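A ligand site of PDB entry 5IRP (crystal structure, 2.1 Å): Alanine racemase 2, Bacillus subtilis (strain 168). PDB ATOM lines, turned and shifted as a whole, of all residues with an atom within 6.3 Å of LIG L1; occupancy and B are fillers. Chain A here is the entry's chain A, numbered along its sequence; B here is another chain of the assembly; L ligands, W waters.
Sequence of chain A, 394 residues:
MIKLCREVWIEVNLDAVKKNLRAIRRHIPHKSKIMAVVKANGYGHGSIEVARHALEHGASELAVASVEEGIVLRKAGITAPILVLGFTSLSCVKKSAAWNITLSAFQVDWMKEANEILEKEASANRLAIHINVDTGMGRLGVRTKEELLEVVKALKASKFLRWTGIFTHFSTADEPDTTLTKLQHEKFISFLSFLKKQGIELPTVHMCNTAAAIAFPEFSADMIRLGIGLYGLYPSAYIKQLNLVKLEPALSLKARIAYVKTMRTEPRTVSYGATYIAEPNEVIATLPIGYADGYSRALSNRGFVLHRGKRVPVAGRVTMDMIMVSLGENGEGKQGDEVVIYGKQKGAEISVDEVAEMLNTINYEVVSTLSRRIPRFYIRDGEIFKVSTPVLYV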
ATOM      1  N   VAL A  37     -14.348  14.034  33.092  1.00  0.00           N
ATOM      2  CA  VAL A  37     -13.625  15.106  32.410  1.00  0.00           C
ATOM      3  C   VAL A  37     -12.890  15.927  33.471  1.00  0.00           C
ATOM      4  O   VAL A  37     -13.504  16.642  34.256  1.00  0.00           O
ATOM      5  CB  VAL A  37     -14.549  15.988  31.569  1.00  0.00           C
ATOM      6  CG1 VAL A  37     -13.724  17.026  30.798  1.00  0.00           C
ATOM      7  CG2 VAL A  37     -15.382  15.144  30.602  1.00  0.00           C
ATOM      8  N   LYS A  39     -10.083  17.977  32.725  1.00  0.00           N
ATOM      9  CA  LYS A  39      -9.233  18.977  32.092  1.00  0.00           C
ATOM     10  C   LYS A  39      -9.179  20.240  32.941  1.00  0.00           C
ATOM     11  O   LYS A  39      -9.992  20.457  33.856  1.00  0.00           O
ATOM     12  CB  LYS A  39      -9.738  19.302  30.686  1.00  0.00           C
ATOM     13  CG  LYS A  39     -11.149  19.925  30.620  1.00  0.00           C
ATOM     14  CD  LYS A  39     -11.767  19.649  29.247  1.00  0.00           C
ATOM     15  CE  LYS A  39     -13.036  20.454  29.014  1.00  0.00           C
ATOM     16  NZ  LYS A  39     -12.698  21.834  28.599  1.00  0.00           N
ATOM     17  N   TYR A  43     -11.213  21.179  36.415  1.00  0.00           N
ATOM     18  CA  TYR A  43     -12.055  22.367  36.494  1.00  0.00           C
ATOM     19  C   TYR A  43     -11.697  23.209  37.716  1.00  0.00           C
ATOM     20  O   TYR A  43     -12.564  23.726  38.413  1.00  0.00           O
ATOM     21  CB  TYR A  43     -13.547  21.999  36.530  1.00  0.00           C
ATOM     22  CG  TYR A  43     -14.193  21.525  35.243  1.00  0.00           C
ATOM     23  CD1 TYR A  43     -13.525  20.697  34.348  1.00  0.00           C
ATOM     24  CD2 TYR A  43     -15.520  21.860  34.948  1.00  0.00           C
ATOM     25  CE1 TYR A  43     -14.147  20.238  33.177  1.00  0.00           C
ATOM     26  CE2 TYR A  43     -16.140  21.430  33.801  1.00  0.00           C
ATOM     27  CZ  TYR A  43     -15.446  20.619  32.916  1.00  0.00           C
ATOM     28  OH  TYR A  43     -16.072  20.179  31.760  1.00  0.00           O
ATOM     29  N   LEU A  85      -8.715  15.751  24.414  1.00  0.00           N
ATOM     30  CA  LEU A  85      -9.890  16.231  23.660  1.00  0.00           C
ATOM     31  C   LEU A  85      -9.539  17.241  22.576  1.00  0.00           C
ATOM     32  O   LEU A  85     -10.292  17.398  21.607  1.00  0.00           O
ATOM     33  CB  LEU A  85     -10.904  16.867  24.616  1.00  0.00           C
ATOM     34  CG  LEU A  85     -11.655  15.957  25.598  1.00  0.00           C
ATOM     35  CD1 LEU A  85     -12.475  16.811  26.587  1.00  0.00           C
ATOM     36  CD2 LEU A  85     -12.563  14.996  24.845  1.00  0.00           C
ATOM     37  N   ASN A 132     -12.765  12.558  16.154  1.00  0.00           N
ATOM     38  CA  ASN A 132     -13.741  13.601  16.433  1.00  0.00           C
ATOM     39  C   ASN A 132     -14.553  13.894  15.171  1.00  0.00           C
ATOM     40  O   ASN A 132     -13.989  14.236  14.129  1.00  0.00           O
ATOM     41  CB  ASN A 132     -13.030  14.870  16.921  1.00  0.00           C
ATOM     42  CG  ASN A 132     -13.998  15.974  17.354  1.00  0.00           C
ATOM     43  OD1 ASN A 132     -15.199  15.936  17.067  1.00  0.00           O
ATOM     44  ND2 ASN A 132     -13.464  16.973  18.046  1.00  0.00           N
ATOM     45  N   ARG A 139     -15.603  23.343  16.036  1.00  0.00           N
ATOM     46  CA  ARG A 139     -14.342  23.581  16.734  1.00  0.00           C
ATOM     47  C   ARG A 139     -13.250  22.676  16.148  1.00  0.00           C
ATOM     48  O   ARG A 139     -12.357  23.153  15.431  1.00  0.00           O
ATOM     49  CB  ARG A 139     -14.511  23.340  18.245  1.00  0.00           C
ATOM     50  CG  ARG A 139     -13.317  23.750  19.119  1.00  0.00           C
ATOM     51  CD  ARG A 139     -13.692  23.750  20.599  1.00  0.00           C
ATOM     52  NE  ARG A 139     -14.293  22.473  20.997  1.00  0.00           N
ATOM     53  CZ  ARG A 139     -14.718  22.197  22.223  1.00  0.00           C
ATOM     54  NH1 ARG A 139     -14.618  23.101  23.177  1.00  0.00           N
ATOM     55  NH2 ARG A 139     -15.255  21.000  22.498  1.00  0.00           N
ATOM     56  N   PHE A 167     -16.429  10.237  18.469  1.00  0.00           N
ATOM     57  CA  PHE A 167     -17.265  11.103  19.274  1.00  0.00           C
ATOM     58  C   PHE A 167     -17.656  12.375  18.522  1.00  0.00           C
ATOM     59  O   PHE A 167     -17.079  12.732  17.479  1.00  0.00           O
ATOM     60  CB  PHE A 167     -16.579  11.449  20.599  1.00  0.00           C
ATOM     61  CG  PHE A 167     -15.356  12.329  20.487  1.00  0.00           C
ATOM     62  CD1 PHE A 167     -14.108  11.773  20.228  1.00  0.00           C
ATOM     63  CD2 PHE A 167     -15.454  13.703  20.687  1.00  0.00           C
ATOM     64  CE1 PHE A 167     -12.964  12.579  20.151  1.00  0.00           C
ATOM     65  CE2 PHE A 167     -14.317  14.515  20.608  1.00  0.00           C
ATOM     66  CZ  PHE A 167     -13.075  13.950  20.341  1.00  0.00           C
ATOM     67  N   THR A 168     -18.675  13.046  19.063  1.00  0.00           N
ATOM     68  CA  THR A 168     -19.007  14.406  18.685  1.00  0.00           C
ATOM     69  C   THR A 168     -19.382  15.175  19.946  1.00  0.00           C
ATOM     70  O   THR A 168     -19.598  14.598  21.021  1.00  0.00           O
ATOM     71  CB  THR A 168     -20.137  14.467  17.645  1.00  0.00           C
ATOM     72  OG1 THR A 168     -20.178  15.773  17.069  1.00  0.00           O
ATOM     73  CG2 THR A 168     -21.485  14.127  18.272  1.00  0.00           C
ATOM     74  N   HIS A 169     -19.455  16.495  19.810  1.00  0.00           N
ATOM     75  CA  HIS A 169     -19.764  17.406  20.902  1.00  0.00           C
ATOM     76  C   HIS A 169     -20.985  18.237  20.535  1.00  0.00           C
ATOM     77  O   HIS A 169     -21.062  18.766  19.423  1.00  0.00           O
ATOM     78  CB  HIS A 169     -18.571  18.312  21.217  1.00  0.00           C
ATOM     79  CG  HIS A 169     -18.613  18.907  22.587  1.00  0.00           C
ATOM     80  ND1 HIS A 169     -18.696  18.133  23.732  1.00  0.00           N
ATOM     81  CD2 HIS A 169     -18.581  20.195  23.009  1.00  0.00           C
ATOM     82  CE1 HIS A 169     -18.725  18.920  24.787  1.00  0.00           C
ATOM     83  NE2 HIS A 169     -18.651  20.177  24.378  1.00  0.00           N
ATOM     84  N   CYS A 208     -22.450  12.513  24.730  1.00  0.00           N
ATOM     85  CA  CYS A 208     -23.072  13.365  25.742  1.00  0.00           C
ATOM     86  C   CYS A 208     -22.044  14.024  26.641  1.00  0.00           C
ATOM     87  O   CYS A 208     -21.137  13.361  27.165  1.00  0.00           O
ATOM     88  CB  CYS A 208     -24.031  12.554  26.623  1.00  0.00           C
ATOM     89  SG  CYS A 208     -25.499  11.979  25.795  1.00  0.00           S
ATOM     90  N   ASN A 209     -22.199  15.339  26.816  1.00  0.00           N
ATOM     91  CA  ASN A 209     -21.678  16.102  27.938  1.00  0.00           C
ATOM     92  C   ASN A 209     -22.656  15.976  29.108  1.00  0.00           C
ATOM     93  O   ASN A 209     -23.631  15.232  29.031  1.00  0.00           O
ATOM     94  CB  ASN A 209     -21.417  17.567  27.520  1.00  0.00           C
ATOM     95  CG  ASN A 209     -22.625  18.238  26.715  1.00  0.00           C
ATOM     96  OD1 ASN A 209     -23.759  17.733  26.625  1.00  0.00           O
ATOM     97  ND2 ASN A 209     -22.327  19.422  26.132  1.00  0.00           N
ATOM     98  N   THR A 210     -22.423  16.703  30.211  1.00  0.00           N
ATOM     99  CA  THR A 210     -23.371  16.665  31.322  1.00  0.00           C
ATOM    100  C   THR A 210     -24.782  17.010  30.874  1.00  0.00           C
ATOM    101  O   THR A 210     -25.745  16.306  31.217  1.00  0.00           O
ATOM    102  CB  THR A 210     -22.926  17.621  32.437  1.00  0.00           C
ATOM    103  OG1 THR A 210     -21.615  17.274  32.889  1.00  0.00           O
ATOM    104  CG2 THR A 210     -23.887  17.546  33.607  1.00  0.00           C
ATOM    105  N   ALA A 211     -24.941  18.080  30.096  1.00  0.00           N
ATOM    106  CA  ALA A 211     -26.278  18.539  29.717  1.00  0.00           C
ATOM    107  C   ALA A 211     -27.061  17.439  29.008  1.00  0.00           C
ATOM    108  O   ALA A 211     -28.188  17.123  29.406  1.00  0.00           O
ATOM    109  CB  ALA A 211     -26.196  19.786  28.832  1.00  0.00           C
ATOM    110  N   ARG A 225     -19.366  11.754  28.618  1.00  0.00           N
ATOM    111  CA  ARG A 225     -18.275  12.554  29.139  1.00  0.00           C
ATOM    112  C   ARG A 225     -18.854  13.454  30.219  1.00  0.00           C
ATOM    113  O   ARG A 225     -19.523  14.450  29.915  1.00  0.00           O
ATOM    114  CB  ARG A 225     -17.595  13.354  28.015  1.00  0.00           C
ATOM    115  CG  ARG A 225     -17.089  12.462  26.889  1.00  0.00           C
ATOM    116  CD  ARG A 225     -16.272  13.240  25.867  1.00  0.00           C
ATOM    117  NE  ARG A 225     -17.025  14.310  25.229  1.00  0.00           N
ATOM    118  CZ  ARG A 225     -17.822  14.159  24.171  1.00  0.00           C
ATOM    119  NH1 ARG A 225     -17.977  12.974  23.621  1.00  0.00           N
ATOM    120  NH2 ARG A 225     -18.451  15.210  23.673  1.00  0.00           N
ATOM    121  N   LEU A 226     -18.610  13.097  31.474  1.00  0.00           N
ATOM    122  CA  LEU A 226     -19.151  13.844  32.609  1.00  0.00           C
ATOM    123  C   LEU A 226     -18.131  14.879  33.060  1.00  0.00           C
ATOM    124  O   LEU A 226     -17.084  14.541  33.643  1.00  0.00           O
ATOM    125  CB  LEU A 226     -19.522  12.898  33.747  1.00  0.00           C
ATOM    126  CG  LEU A 226     -20.107  13.610  34.955  1.00  0.00           C
ATOM    127  CD1 LEU A 226     -21.462  14.253  34.611  1.00  0.00           C
ATOM    128  CD2 LEU A 226     -20.236  12.635  36.121  1.00  0.00           C
ATOM    129  N   GLY A 227     -18.443  16.151  32.822  1.00  0.00           N
ATOM    130  CA  GLY A 227     -17.603  17.241  33.251  1.00  0.00           C
ATOM    131  C   GLY A 227     -18.197  17.998  34.405  1.00  0.00           C
ATOM    132  O   GLY A 227     -18.084  17.576  35.560  1.00  0.00           O
ATOM    133  N   ILE A 228     -18.860  19.123  34.092  1.00  0.00           N
ATOM    134  CA  ILE A 228     -19.333  20.057  35.120  1.00  0.00           C
ATOM    135  C   ILE A 228     -20.154  19.341  36.188  1.00  0.00           C
ATOM    136  O   ILE A 228     -20.065  19.679  37.383  1.00  0.00           O
ATOM    137  CB  ILE A 228     -20.130  21.206  34.454  1.00  0.00           C
ATOM    138  CG1 ILE A 228     -20.384  22.332  35.461  1.00  0.00           C
ATOM    139  CG2 ILE A 228     -21.467  20.708  33.860  1.00  0.00           C
ATOM    140  CD1 ILE A 228     -19.130  23.106  35.860  1.00  0.00           C
ATOM    141  N   GLY A 229     -20.942  18.343  35.798  1.00  0.00           N
ATOM    142  CA  GLY A 229     -21.790  17.656  36.751  1.00  0.00           C
ATOM    143  C   GLY A 229     -21.016  16.860  37.785  1.00  0.00           C
ATOM    144  O   GLY A 229     -21.502  16.658  38.910  1.00  0.00           O
ATOM    145  N   PRO A 235     -24.813  22.418  33.993  1.00  0.00           N
ATOM    146  CA  PRO A 235     -24.382  23.153  32.792  1.00  0.00           C
ATOM    147  C   PRO A 235     -25.206  24.400  32.494  1.00  0.00           C
ATOM    148  O   PRO A 235     -24.724  25.282  31.787  1.00  0.00           O
ATOM    149  CB  PRO A 235     -24.532  22.115  31.663  1.00  0.00           C
ATOM    150  CG  PRO A 235     -25.522  21.099  32.193  1.00  0.00           C
ATOM    151  CD  PRO A 235     -25.307  21.061  33.678  1.00  0.00           C
ATOM    152  N   TYR A 364     -18.592  27.206  35.034  1.00  0.00           N
ATOM    153  CA  TYR A 364     -17.350  26.629  34.487  1.00  0.00           C
ATOM    154  C   TYR A 364     -16.164  27.581  34.643  1.00  0.00           C
ATOM    155  O   TYR A 364     -15.053  27.167  35.026  1.00  0.00           O
ATOM    156  CB  TYR A 364     -17.481  26.304  33.000  1.00  0.00           C
ATOM    157  CG  TYR A 364     -18.484  25.279  32.528  1.00  0.00           C
ATOM    158  CD1 TYR A 364     -19.850  25.578  32.506  1.00  0.00           C
ATOM    159  CD2 TYR A 364     -18.072  24.063  31.987  1.00  0.00           C
ATOM    160  CE1 TYR A 364     -20.780  24.661  32.020  1.00  0.00           C
ATOM    161  CE2 TYR A 364     -19.002  23.132  31.504  1.00  0.00           C
ATOM    162  CZ  TYR A 364     -20.353  23.450  31.522  1.00  0.00           C
ATOM    163  OH  TYR A 364     -21.294  22.557  31.049  1.00  0.00           O
ATOM    164  N   TYR B 272     -20.129  27.139  21.470  1.00  0.00           N
ATOM    165  CA  TYR B 272     -21.293  26.937  22.335  1.00  0.00           C
ATOM    166  C   TYR B 272     -22.343  28.016  22.092  1.00  0.00           C
ATOM    167  O   TYR B 272     -22.043  29.162  21.707  1.00  0.00           O
ATOM    168  CB  TYR B 272     -20.863  26.932  23.806  1.00  0.00           C
ATOM    169  CG  TYR B 272     -20.154  25.668  24.255  1.00  0.00           C
ATOM    170  CD1 TYR B 272     -20.765  24.424  24.143  1.00  0.00           C
ATOM    171  CD2 TYR B 272     -18.883  25.722  24.832  1.00  0.00           C
ATOM    172  CE1 TYR B 272     -20.138  23.273  24.561  1.00  0.00           C
ATOM    173  CE2 TYR B 272     -18.241  24.572  25.252  1.00  0.00           C
ATOM    174  CZ  TYR B 272     -18.887  23.344  25.120  1.00  0.00           C
ATOM    175  OH  TYR B 272     -18.286  22.175  25.527  1.00  0.00           O
ATOM    176  N   MET B 320     -13.435  26.406  27.265  1.00  0.00           N
ATOM    177  CA  MET B 320     -12.518  26.305  28.404  1.00  0.00           C
ATOM    178  C   MET B 320     -11.060  26.232  27.948  1.00  0.00           C
ATOM    179  O   MET B 320     -10.180  26.840  28.574  1.00  0.00           O
ATOM    180  CB  MET B 320     -12.874  25.103  29.274  1.00  0.00           C
ATOM    181  CG  MET B 320     -11.961  24.986  30.499  1.00  0.00           C
ATOM    182  SD  MET B 320     -12.409  23.646  31.616  1.00  0.00           S
ATOM    183  CE  MET B 320     -14.116  24.106  32.019  1.00  0.00           C
ATOM    184  N   ASP B 321     -10.793  25.533  26.839  1.00  0.00           N
ATOM    185  CA  ASP B 321      -9.436  25.333  26.356  1.00  0.00           C
ATOM    186  C   ASP B 321      -9.191  25.825  24.932  1.00  0.00           C
ATOM    187  O   ASP B 321      -8.053  25.746  24.465  1.00  0.00           O
ATOM    188  CB  ASP B 321      -9.082  23.843  26.414  1.00  0.00           C
ATOM    189  CG  ASP B 321      -9.532  23.200  27.695  1.00  0.00           C
ATOM    190  OD1 ASP B 321      -9.164  23.706  28.770  1.00  0.00           O
ATOM    191  OD2 ASP B 321     -10.266  22.194  27.618  1.00  0.00           O
ATOM    192  N   MET B 322     -10.209  26.317  24.233  1.00  0.00           N
ATOM    193  CA  MET B 322     -10.057  26.609  22.810  1.00  0.00           C
ATOM    194  C   MET B 322     -10.889  27.829  22.435  1.00  0.00           C
ATOM    195  O   MET B 322     -11.926  28.101  23.048  1.00  0.00           O
ATOM    196  CB  MET B 322     -10.471  25.414  21.937  1.00  0.00           C
ATOM    197  CG  MET B 322      -9.389  24.366  21.770  1.00  0.00           C
ATOM    198  SD  MET B 322      -9.923  22.981  20.735  1.00  0.00           S
ATOM    199  CE  MET B 322     -10.752  21.946  21.953  1.00  0.00           C
HETATM  200  C1  LIG L   1     -15.282  17.640  23.908  1.00  0.00           C
HETATM  201  C2  LIG L   1     -15.779  17.842  25.339  1.00  0.00           C
HETATM  202  C3  LIG L   1     -15.406  18.956  26.100  1.00  0.00           C
HETATM  203  O1  LIG L   1     -14.547  19.928  25.559  1.00  0.00           O
HETATM  204  C4  LIG L   1     -15.885  19.102  27.392  1.00  0.00           C
HETATM  205  C5  LIG L   1     -16.725  18.124  27.906  1.00  0.00           C
HETATM  206  C6  LIG L   1     -17.314  18.232  29.324  1.00  0.00           C
HETATM  207  O2  LIG L   1     -18.482  19.008  29.198  1.00  0.00           O
HETATM  208  P1  LIG L   1     -19.484  19.415  30.463  1.00  0.00           P
HETATM  209  O3  LIG L   1     -20.656  20.441  29.910  1.00  0.00           O
HETATM  210  O4  LIG L   1     -18.748  20.034  31.562  1.00  0.00           O
HETATM  211  O5  LIG L   1     -20.025  18.260  31.164  1.00  0.00           O
HETATM  212  C7  LIG L   1     -17.058  17.051  27.100  1.00  0.00           C
HETATM  213  N1  LIG L   1     -16.577  16.936  25.874  1.00  0.00           N
HETATM  214  C1  LG2 L   2     -15.392  23.131  26.377  1.00  0.00           C
HETATM  215  O1  LG2 L   2     -15.692  22.222  25.610  1.00  0.00           O
HETATM  216  O2  LG2 L   2     -15.091  24.037  27.135  1.00  0.00           O
HETATM  217  O   HOH W   1     -20.531  21.519  27.405  1.00  0.00           O
HETATM  218  O   HOH W   2     -12.826  18.637  21.763  1.00  0.00           O
HETATM  219  O   HOH W   3     -23.037  19.986  29.421  1.00  0.00           O
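An oxygen (O3) of LIG L1 lies within hydrogen-bond range of the side-chain hydroxyl of Tyr 364, 2.5 Å away. O5 of LIG L1 is in hydrogen-bond range of N of Thr 210 (3.0 Å). An oxygen (O5) of LIG L1 is in hydrogen-bond range of the side-chain hydroxyl (OG1) of Thr 210 (2.5 Å). The side-chain hydroxyl (OH) of Tyr 43 is in hydrogen-bond range of an oxygen (O4) of LIG L1 (2.7 Å). O4 of LIG L1 is in hydrogen-bond range of N of Ile 228 (2.7 Å). NE of Arg 225 is in hydrogen-bond range of N1 of LIG L1, 2.7 Å away. An oxygen (O5) of LIG L1 lies within hydrogen-bond range of the backbone NH (N) of Gly 227, at 3.1 Å. N1 of LIG L1 lies close to ND1 of His 169. NH2 of Arg 139 is in hydrogen-bond range of O1 of LIG L1. An oxygen (O1) of LG2 L2 is in hydrogen-bond range of the guanidinium group of Arg 139 (2.8 Å). The side-chain hydroxyl (OH) of Tyr 272 of chain B lies within hydrogen-bond range of an oxygen (O1) of LG2 L2. N of Met 320 of chain B is in hydrogen-bond range of O2 of LG2 L2, at 2.9 Å.
An oxygen (O1) of LG2 L2 sits at hydrogen-bond distance from an oxygen (O1) of LIG L1 (2.6 Å).
OG1 of Thr 210 is in hydrogen-bond range of N of Gly 227 (3.4 Å). The backbone NH (N) of Gly 229 sits at hydrogen-bond distance from the side-chain hydroxyl (OG1) of Thr 210 (3.2 Å). A ring nitrogen (ND1) of His 169 lies within hydrogen-bond range of the guanidinium group (NH2) of Arg 225 (2.9 Å). The backbone NH (N) of Arg 225 is in hydrogen-bond range of the backbone carbonyl oxygen (O) of Cys 208 (2.8 Å). NH2 of Arg 225 is in hydrogen-bond range of O of Thr 168 (3.0 Å). The side-chain amino group of Lys 39 is in salt-bridge range of the side-chain carboxylate of Asp 321 of chain B, at 2.6 Å. The side-chain amino group (NZ) of Lys 39 sits close to the side-chain sulfur (SD) of Met 320 of chain B. N of Val 37 sits at hydrogen-bond distance from O of Leu 226 (2.8 Å).
CG2 of Val 37 touches C6 of LIG L1, 3.9 Å away. Lys 39 touches LIG L1. Leu 85 touches LIG L1 (CD1 to C3, 3.7 Å). Asn 209 touches LIG L1 (CB to O2, 3.7 Å). Hydrophobic or aromatic side chains that line LIG L1: Val 37, Tyr 43, Leu 85, His 169, Ile 228 and Tyr 364. 12 residues have an atom within 4 Å of LIG L1: Val 37, Lys 39, Tyr 43, Leu 85, Arg 139, His 169, Asn 209, Thr 210, Arg 225, Gly 227, Ile 228 and Tyr 364.
Water W1 lies within hydrogen-bond range of O3 of LIG L1 (2.7 Å), OH of Tyr 272 of chain B (3.0 Å) and ND2 of Asn 209 (3.0 Å). Water W2 bridges the backbone carbonyl oxygen of Leu 85 and the guanidinium group of Arg 139.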
